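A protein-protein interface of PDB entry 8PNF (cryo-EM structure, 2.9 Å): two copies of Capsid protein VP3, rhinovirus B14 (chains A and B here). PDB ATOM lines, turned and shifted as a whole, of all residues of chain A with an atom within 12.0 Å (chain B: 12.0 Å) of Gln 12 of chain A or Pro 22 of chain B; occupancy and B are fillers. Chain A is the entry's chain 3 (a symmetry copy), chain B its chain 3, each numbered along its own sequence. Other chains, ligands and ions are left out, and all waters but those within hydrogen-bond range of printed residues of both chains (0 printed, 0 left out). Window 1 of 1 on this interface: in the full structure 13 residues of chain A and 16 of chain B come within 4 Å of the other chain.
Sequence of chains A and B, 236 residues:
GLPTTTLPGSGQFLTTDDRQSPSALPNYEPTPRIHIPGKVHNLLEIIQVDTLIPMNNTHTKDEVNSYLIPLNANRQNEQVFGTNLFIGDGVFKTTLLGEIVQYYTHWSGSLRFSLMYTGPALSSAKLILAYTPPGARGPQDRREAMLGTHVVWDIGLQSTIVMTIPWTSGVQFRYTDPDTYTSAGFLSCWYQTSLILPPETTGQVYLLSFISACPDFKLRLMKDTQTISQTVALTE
The backbone carbonyl oxygen of Ala 24 of chain B is in hydrogen-bond range of the side-chain hydroxyl of Thr 16 of chain A, 3.5 Å away.
O of Thr 6 of chain A lies within hydrogen-bond range of N of Gly 11 of chain B (2.8 Å).
Among the printed residues, merely in contact across the chains: Pro 8 of chain A with Gln 12 of chain B (3.4 Å) and Gln 12 of chain A with Pro 22 of chain B (3.9 Å).
Gln 12 of chain A touches just one residue of chain B: Pro 22.
Printed residues of chain A within 4 Å of Pro 22 of chain B: Gln 12 (3.9 Å).
No residue of chain B comes within 4 Å of Ser 10 of chain A.
No residue of chain A comes within 4 Å of Ser 21 of chain B.
No residue of chain A comes within 4 Å of Ser 23 of chain B.
Of chain A, only Thr 16 comes within 4 Å of Ala 24 of chain B.
Printed residues of chain B within 4 Å of Pro 8 of chain A: Gln 12 (3.4 Å).
Printed residues of chain A within 4 Å of Gln 12 of chain B: Pro 8.
Of the 14 printed residues of chain B, 4 touch a printed residue of chain A.
Hydrophobic or aromatic side chains of chain B that line the printed part of chain A: Pro 22.
Hydrophobic or aromatic side chains of chain A within 4 Å of the printed part of chain B: Pro 8.
Positions printed for both chains: 11, 12, 13, 18, 19, 20 and 21.
Of the 4 pairs that touch across the chains among the printed residues, none has its exchanged pair printed and touching as well.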
ATOM      1  N   THR A   6      14.097   2.118  31.757  1.00  0.00           N
ATOM      2  CA  THR A   6      15.252   2.055  30.873  1.00  0.00           C
ATOM      3  C   THR A   6      15.076   0.931  29.863  1.00  0.00           C
ATOM      4  O   THR A   6      14.699  -0.188  30.222  1.00  0.00           O
ATOM      5  CB  THR A   6      16.545   1.854  31.663  1.00  0.00           C
ATOM      6  OG1 THR A   6      16.382   0.777  32.588  1.00  0.00           O
ATOM      7  CG2 THR A   6      16.904   3.118  32.418  1.00  0.00           C
ATOM      8  N   LEU A   7      15.357   1.238  28.607  1.00  0.00           N
ATOM      9  CA  LEU A   7      15.116   0.359  27.480  1.00  0.00           C
ATOM     10  C   LEU A   7      16.314  -0.550  27.230  1.00  0.00           C
ATOM     11  O   LEU A   7      17.404  -0.304  27.748  1.00  0.00           O
ATOM     12  CB  LEU A   7      14.809   1.208  26.248  1.00  0.00           C
ATOM     13  CG  LEU A   7      13.503   2.005  26.282  1.00  0.00           C
ATOM     14  CD1 LEU A   7      13.171   2.522  24.905  1.00  0.00           C
ATOM     15  CD2 LEU A   7      12.358   1.166  26.820  1.00  0.00           C
ATOM     16  N   PRO A   8      16.132  -1.644  26.481  1.00  0.00           N
ATOM     17  CA  PRO A   8      17.295  -2.412  26.023  1.00  0.00           C
ATOM     18  C   PRO A   8      18.150  -1.601  25.065  1.00  0.00           C
ATOM     19  O   PRO A   8      17.667  -1.059  24.069  1.00  0.00           O
ATOM     20  CB  PRO A   8      16.673  -3.630  25.331  1.00  0.00           C
ATOM     21  CG  PRO A   8      15.265  -3.278  25.110  1.00  0.00           C
ATOM     22  CD  PRO A   8      14.884  -2.384  26.228  1.00  0.00           C
ATOM     23  N   GLY A   9      19.435  -1.523  25.379  1.00  0.00           N
ATOM     24  CA  GLY A   9      20.320  -0.590  24.727  1.00  0.00           C
ATOM     25  C   GLY A   9      20.737   0.575  25.588  1.00  0.00           C
ATOM     26  O   GLY A   9      21.283   1.547  25.059  1.00  0.00           O
ATOM     27  N   SER A  10      20.478   0.518  26.890  1.00  0.00           N
ATOM     28  CA  SER A  10      20.950   1.534  27.816  1.00  0.00           C
ATOM     29  C   SER A  10      22.390   1.225  28.196  1.00  0.00           C
ATOM     30  O   SER A  10      22.699   0.110  28.623  1.00  0.00           O
ATOM     31  CB  SER A  10      20.060   1.586  29.051  1.00  0.00           C
ATOM     32  OG  SER A  10      18.703   1.707  28.689  1.00  0.00           O
ATOM     33  N   GLY A  11      23.267   2.208  28.039  1.00  0.00           N
ATOM     34  CA  GLY A  11      24.676   2.018  28.290  1.00  0.00           C
ATOM     35  C   GLY A  11      25.460   1.475  27.122  1.00  0.00           C
ATOM     36  O   GLY A  11      26.657   1.214  27.275  1.00  0.00           O
ATOM     37  N   GLN A  12      24.826   1.272  25.970  1.00  0.00           N
ATOM     38  CA  GLN A  12      25.561   0.850  24.792  1.00  0.00           C
ATOM     39  C   GLN A  12      26.300   2.035  24.185  1.00  0.00           C
ATOM     40  O   GLN A  12      25.938   3.199  24.377  1.00  0.00           O
ATOM     41  CB  GLN A  12      24.624   0.220  23.761  1.00  0.00           C
ATOM     42  CG  GLN A  12      23.837   1.206  22.924  1.00  0.00           C
ATOM     43  CD  GLN A  12      22.978   0.532  21.886  1.00  0.00           C
ATOM     44  OE1 GLN A  12      22.912  -0.690  21.823  1.00  0.00           O
ATOM     45  NE2 GLN A  12      22.303   1.327  21.072  1.00  0.00           N
ATOM     46  N   PHE A  13      27.375   1.727  23.472  1.00  0.00           N
ATOM     47  CA  PHE A  13      28.133   2.721  22.722  1.00  0.00           C
ATOM     48  C   PHE A  13      27.991   2.353  21.251  1.00  0.00           C
ATOM     49  O   PHE A  13      28.675   1.455  20.754  1.00  0.00           O
ATOM     50  CB  PHE A  13      29.593   2.770  23.186  1.00  0.00           C
ATOM     51  CG  PHE A  13      30.524   3.477  22.233  1.00  0.00           C
ATOM     52  CD1 PHE A  13      30.233   4.744  21.751  1.00  0.00           C
ATOM     53  CD2 PHE A  13      31.703   2.875  21.835  1.00  0.00           C
ATOM     54  CE1 PHE A  13      31.086   5.378  20.874  1.00  0.00           C
ATOM     55  CE2 PHE A  13      32.559   3.513  20.974  1.00  0.00           C
ATOM     56  CZ  PHE A  13      32.247   4.762  20.490  1.00  0.00           C
ATOM     57  N   LEU A  14      27.089   3.045  20.564  1.00  0.00           N
ATOM     58  CA  LEU A  14      26.978   2.965  19.116  1.00  0.00           C
ATOM     59  C   LEU A  14      27.848   4.055  18.505  1.00  0.00           C
ATOM     60  O   LEU A  14      27.709   5.230  18.858  1.00  0.00           O
ATOM     61  CB  LEU A  14      25.523   3.127  18.678  1.00  0.00           C
ATOM     62  CG  LEU A  14      25.151   2.915  17.208  1.00  0.00           C
ATOM     63  CD1 LEU A  14      25.684   1.601  16.678  1.00  0.00           C
ATOM     64  CD2 LEU A  14      23.653   2.990  17.029  1.00  0.00           C
ATOM     65  N   THR A  15      28.741   3.660  17.593  1.00  0.00           N
ATOM     66  CA  THR A  15      29.698   4.605  17.028  1.00  0.00           C
ATOM     67  C   THR A  15      29.028   5.624  16.118  1.00  0.00           C
ATOM     68  O   THR A  15      29.530   6.744  15.973  1.00  0.00           O
ATOM     69  CB  THR A  15      30.791   3.866  16.256  1.00  0.00           C
ATOM     70  OG1 THR A  15      30.231   3.268  15.083  1.00  0.00           O
ATOM     71  CG2 THR A  15      31.423   2.792  17.112  1.00  0.00           C
ATOM     72  N   THR A  16      27.901   5.273  15.516  1.00  0.00           N
ATOM     73  CA  THR A  16      27.200   6.164  14.607  1.00  0.00           C
ATOM     74  C   THR A  16      26.130   6.997  15.298  1.00  0.00           C
ATOM     75  O   THR A  16      25.399   7.724  14.622  1.00  0.00           O
ATOM     76  CB  THR A  16      26.578   5.363  13.468  1.00  0.00           C
ATOM     77  OG1 THR A  16      25.921   4.213  14.002  1.00  0.00           O
ATOM     78  CG2 THR A  16      27.647   4.912  12.517  1.00  0.00           C
ATOM     79  N   ASP A  17      26.020   6.910  16.620  1.00  0.00           N
ATOM     80  CA  ASP A  17      25.010   7.664  17.345  1.00  0.00           C
ATOM     81  C   ASP A  17      25.391   9.138  17.419  1.00  0.00           C
ATOM     82  O   ASP A  17      26.528   9.484  17.749  1.00  0.00           O
ATOM     83  CB  ASP A  17      24.824   7.099  18.747  1.00  0.00           C
ATOM     84  CG  ASP A  17      23.372   7.062  19.163  1.00  0.00           C
ATOM     85  OD1 ASP A  17      22.606   7.925  18.695  1.00  0.00           O
ATOM     86  OD2 ASP A  17      22.990   6.166  19.945  1.00  0.00           O
ATOM     87  N   ASP A  18      24.427  10.003  17.123  1.00  0.00           N
ATOM     88  CA  ASP A  18      24.621  11.446  17.031  1.00  0.00           C
ATOM     89  C   ASP A  18      23.812  12.114  18.135  1.00  0.00           C
ATOM     90  O   ASP A  18      22.678  12.545  17.916  1.00  0.00           O
ATOM     91  CB  ASP A  18      24.204  11.923  15.661  1.00  0.00           C
ATOM     92  CG  ASP A  18      24.474  13.385  15.447  1.00  0.00           C
ATOM     93  OD1 ASP A  18      25.433  13.908  16.045  1.00  0.00           O
ATOM     94  OD2 ASP A  18      23.711  14.018  14.690  1.00  0.00           O
ATOM     95  N   ARG A  19      24.395  12.202  19.325  1.00  0.00           N
ATOM     96  CA  ARG A  19      23.743  12.843  20.455  1.00  0.00           C
ATOM     97  C   ARG A  19      24.577  14.020  20.943  1.00  0.00           C
ATOM     98  O   ARG A  19      25.583  14.401  20.342  1.00  0.00           O
ATOM     99  CB  ARG A  19      23.502  11.866  21.613  1.00  0.00           C
ATOM    100  CG  ARG A  19      22.977  10.489  21.242  1.00  0.00           C
ATOM    101  CD  ARG A  19      21.676  10.529  20.458  1.00  0.00           C
ATOM    102  NE  ARG A  19      20.591  11.230  21.127  1.00  0.00           N
ATOM    103  CZ  ARG A  19      19.486  11.635  20.512  1.00  0.00           C
ATOM    104  NH1 ARG A  19      19.326  11.403  19.220  1.00  0.00           N
ATOM    105  NH2 ARG A  19      18.542  12.270  21.185  1.00  0.00           N
ATOM    106  N   GLN A  20      24.126  14.598  22.046  1.00  0.00           N
ATOM    107  CA  GLN A  20      24.843  15.665  22.716  1.00  0.00           C
ATOM    108  C   GLN A  20      25.644  15.097  23.882  1.00  0.00           C
ATOM    109  O   GLN A  20      25.364  14.010  24.392  1.00  0.00           O
ATOM    110  CB  GLN A  20      23.863  16.719  23.213  1.00  0.00           C
ATOM    111  CG  GLN A  20      23.060  17.359  22.111  1.00  0.00           C
ATOM    112  CD  GLN A  20      22.040  18.328  22.637  1.00  0.00           C
ATOM    113  OE1 GLN A  20      21.925  18.525  23.838  1.00  0.00           O
ATOM    114  NE2 GLN A  20      21.279  18.929  21.740  1.00  0.00           N
ATOM    115  N   SER A  21      26.660  15.851  24.305  1.00  0.00           N
ATOM    116  CA  SER A  21      27.544  15.397  25.366  1.00  0.00           C
ATOM    117  C   SER A  21      28.127  16.625  26.038  1.00  0.00           C
ATOM    118  O   SER A  21      28.195  17.679  25.394  1.00  0.00           O
ATOM    119  CB  SER A  21      28.651  14.495  24.808  1.00  0.00           C
ATOM    120  OG  SER A  21      29.675  15.247  24.197  1.00  0.00           O
ATOM    121  N   GLY B  11      15.184  -2.624  31.547  1.00  0.00           N
ATOM    122  CA  GLY B  11      16.160  -3.536  31.000  1.00  0.00           C
ATOM    123  C   GLY B  11      15.596  -4.844  30.505  1.00  0.00           C
ATOM    124  O   GLY B  11      16.372  -5.711  30.089  1.00  0.00           O
ATOM    125  N   GLN B  12      14.281  -5.029  30.557  1.00  0.00           N
ATOM    126  CA  GLN B  12      13.684  -6.228  29.996  1.00  0.00           C
ATOM    127  C   GLN B  12      13.617  -6.117  28.478  1.00  0.00           C
ATOM    128  O   GLN B  12      13.614  -5.026  27.902  1.00  0.00           O
ATOM    129  CB  GLN B  12      12.290  -6.467  30.577  1.00  0.00           C
ATOM    130  CG  GLN B  12      11.190  -5.627  29.965  1.00  0.00           C
ATOM    131  CD  GLN B  12       9.830  -5.947  30.532  1.00  0.00           C
ATOM    132  OE1 GLN B  12       9.704  -6.761  31.439  1.00  0.00           O
ATOM    133  NE2 GLN B  12       8.804  -5.298  30.006  1.00  0.00           N
ATOM    134  N   PHE B  13      13.600  -7.272  27.827  1.00  0.00           N
ATOM    135  CA  PHE B  13      13.418  -7.359  26.383  1.00  0.00           C
ATOM    136  C   PHE B  13      12.098  -8.085  26.158  1.00  0.00           C
ATOM    137  O   PHE B  13      12.030  -9.314  26.240  1.00  0.00           O
ATOM    138  CB  PHE B  13      14.606  -8.058  25.715  1.00  0.00           C
ATOM    139  CG  PHE B  13      14.340  -8.525  24.306  1.00  0.00           C
ATOM    140  CD1 PHE B  13      13.816  -7.669  23.351  1.00  0.00           C
ATOM    141  CD2 PHE B  13      14.635  -9.825  23.936  1.00  0.00           C
ATOM    142  CE1 PHE B  13      13.568  -8.107  22.069  1.00  0.00           C
ATOM    143  CE2 PHE B  13      14.402 -10.257  22.655  1.00  0.00           C
ATOM    144  CZ  PHE B  13      13.864  -9.399  21.723  1.00  0.00           C
ATOM    145  N   ASP B  18       6.925  -2.246  20.923  1.00  0.00           N
ATOM    146  CA  ASP B  18       6.998  -1.421  19.721  1.00  0.00           C
ATOM    147  C   ASP B  18       7.499  -0.037  20.113  1.00  0.00           C
ATOM    148  O   ASP B  18       6.708   0.879  20.343  1.00  0.00           O
ATOM    149  CB  ASP B  18       5.638  -1.363  19.068  1.00  0.00           C
ATOM    150  CG  ASP B  18       5.651  -0.620  17.762  1.00  0.00           C
ATOM    151  OD1 ASP B  18       6.692  -0.633  17.079  1.00  0.00           O
ATOM    152  OD2 ASP B  18       4.619  -0.004  17.428  1.00  0.00           O
ATOM    153  N   ARG B  19       8.815   0.115  20.189  1.00  0.00           N
ATOM    154  CA  ARG B  19       9.423   1.392  20.524  1.00  0.00           C
ATOM    155  C   ARG B  19      10.323   1.859  19.388  1.00  0.00           C
ATOM    156  O   ARG B  19      10.383   1.259  18.313  1.00  0.00           O
ATOM    157  CB  ARG B  19      10.230   1.324  21.827  1.00  0.00           C
ATOM    158  CG  ARG B  19       9.590   0.573  22.984  1.00  0.00           C
ATOM    159  CD  ARG B  19       8.224   1.112  23.372  1.00  0.00           C
ATOM    160  NE  ARG B  19       8.211   2.523  23.724  1.00  0.00           N
ATOM    161  CZ  ARG B  19       7.104   3.253  23.803  1.00  0.00           C
ATOM    162  NH1 ARG B  19       5.929   2.699  23.557  1.00  0.00           N
ATOM    163  NH2 ARG B  19       7.169   4.533  24.126  1.00  0.00           N
ATOM    164  N   GLN B  20      11.017   2.958  19.647  1.00  0.00           N
ATOM    165  CA  GLN B  20      12.001   3.493  18.728  1.00  0.00           C
ATOM    166  C   GLN B  20      13.398   3.055  19.153  1.00  0.00           C
ATOM    167  O   GLN B  20      13.638   2.687  20.305  1.00  0.00           O
ATOM    168  CB  GLN B  20      11.912   5.012  18.695  1.00  0.00           C
ATOM    169  CG  GLN B  20      10.570   5.526  18.243  1.00  0.00           C
ATOM    170  CD  GLN B  20      10.480   7.024  18.306  1.00  0.00           C
ATOM    171  OE1 GLN B  20      11.428   7.691  18.696  1.00  0.00           O
ATOM    172  NE2 GLN B  20       9.332   7.564  17.939  1.00  0.00           N
ATOM    173  N   SER B  21      14.330   3.095  18.201  1.00  0.00           N
ATOM    174  CA  SER B  21      15.688   2.642  18.454  1.00  0.00           C
ATOM    175  C   SER B  21      16.606   3.371  17.493  1.00  0.00           C
ATOM    176  O   SER B  21      16.136   3.797  16.432  1.00  0.00           O
ATOM    177  CB  SER B  21      15.800   1.123  18.282  1.00  0.00           C
ATOM    178  OG  SER B  21      15.872   0.761  16.921  1.00  0.00           O
ATOM    179  N   PRO B  22      17.883   3.574  17.829  1.00  0.00           N
ATOM    180  CA  PRO B  22      18.762   4.338  16.937  1.00  0.00           C
ATOM    181  C   PRO B  22      19.072   3.606  15.643  1.00  0.00           C
ATOM    182  O   PRO B  22      19.251   2.388  15.618  1.00  0.00           O
ATOM    183  CB  PRO B  22      20.026   4.537  17.778  1.00  0.00           C
ATOM    184  CG  PRO B  22      19.973   3.469  18.795  1.00  0.00           C
ATOM    185  CD  PRO B  22      18.530   3.336  19.128  1.00  0.00           C
ATOM    186  N   SER B  23      19.150   4.373  14.562  1.00  0.00           N
ATOM    187  CA  SER B  23      19.449   3.809  13.258  1.00  0.00           C
ATOM    188  C   SER B  23      20.947   3.576  13.122  1.00  0.00           C
ATOM    189  O   SER B  23      21.749   4.495  13.312  1.00  0.00           O
ATOM    190  CB  SER B  23      18.949   4.725  12.148  1.00  0.00           C
ATOM    191  OG  SER B  23      19.064   4.099  10.886  1.00  0.00           O
ATOM    192  N   ALA B  24      21.322   2.341  12.787  1.00  0.00           N
ATOM    193  CA  ALA B  24      22.730   2.008  12.621  1.00  0.00           C
ATOM    194  C   ALA B  24      23.305   2.553  11.322  1.00  0.00           C
ATOM    195  O   ALA B  24      24.528   2.669  11.206  1.00  0.00           O
ATOM    196  CB  ALA B  24      22.928   0.496  12.681  1.00  0.00           C
ATOM    197  N   LEU B  25      22.464   2.900  10.350  1.00  0.00           N
ATOM    198  CA  LEU B  25      22.916   3.472   9.083  1.00  0.00           C
ATOM    199  C   LEU B  25      22.299   4.853   8.944  1.00  0.00           C
ATOM    200  O   LEU B  25      21.215   5.000   8.362  1.00  0.00           O
ATOM    201  CB  LEU B  25      22.535   2.590   7.897  1.00  0.00           C
ATOM    202  CG  LEU B  25      22.789   1.087   7.986  1.00  0.00           C
ATOM    203  CD1 LEU B  25      22.218   0.427   6.766  1.00  0.00           C
ATOM    204  CD2 LEU B  25      24.264   0.773   8.118  1.00  0.00           C
ATOM    205  N   PRO B  26      22.938   5.889   9.477  1.00  0.00           N
ATOM    206  CA  PRO B  26      22.412   7.243   9.312  1.00  0.00           C
ATOM    207  C   PRO B  26      22.558   7.740   7.883  1.00  0.00           C
ATOM    208  O   PRO B  26      23.461   7.337   7.147  1.00  0.00           O
ATOM    209  CB  PRO B  26      23.261   8.070  10.283  1.00  0.00           C
ATOM    210  CG  PRO B  26      24.501   7.307  10.449  1.00  0.00           C
ATOM    211  CD  PRO B  26      24.159   5.867  10.300  1.00  0.00           C
ATOM    212  N   ASN B  27      21.599   8.585   7.494  1.00  0.00           N
ATOM    213  CA  ASN B  27      21.488   9.235   6.186  1.00  0.00           C
ATOM    214  C   ASN B  27      21.326   8.253   5.029  1.00  0.00           C
ATOM    215  O   ASN B  27      21.502   8.631   3.870  1.00  0.00           O
ATOM    216  CB  ASN B  27      22.672  10.171   5.917  1.00  0.00           C
ATOM    217  CG  ASN B  27      22.749  11.299   6.908  1.00  0.00           C
ATOM    218  OD1 ASN B  27      23.605  11.308   7.786  1.00  0.00           O
ATOM    219  ND2 ASN B  27      21.851  12.261   6.775  1.00  0.00           N
ATOM    220  N   TYR B  28      20.958   7.008   5.307  1.00  0.00           N
ATOM    221  CA  TYR B  28      20.787   6.016   4.259  1.00  0.00           C
ATOM    222  C   TYR B  28      19.478   6.254   3.518  1.00  0.00           C
ATOM    223  O   TYR B  28      18.419   6.413   4.132  1.00  0.00           O
ATOM    224  CB  TYR B  28      20.817   4.606   4.853  1.00  0.00           C
ATOM    225  CG  TYR B  28      20.715   3.488   3.836  1.00  0.00           C
ATOM    226  CD1 TYR B  28      21.846   2.995   3.204  1.00  0.00           C
ATOM    227  CD2 TYR B  28      19.488   2.911   3.523  1.00  0.00           C
ATOM    228  CE1 TYR B  28      21.758   1.979   2.279  1.00  0.00           C
ATOM    229  CE2 TYR B  28      19.392   1.899   2.598  1.00  0.00           C
ATOM    230  CZ  TYR B  28      20.529   1.435   1.986  1.00  0.00           C
ATOM    231  OH  TYR B  28      20.424   0.420   1.070  1.00  0.00           O
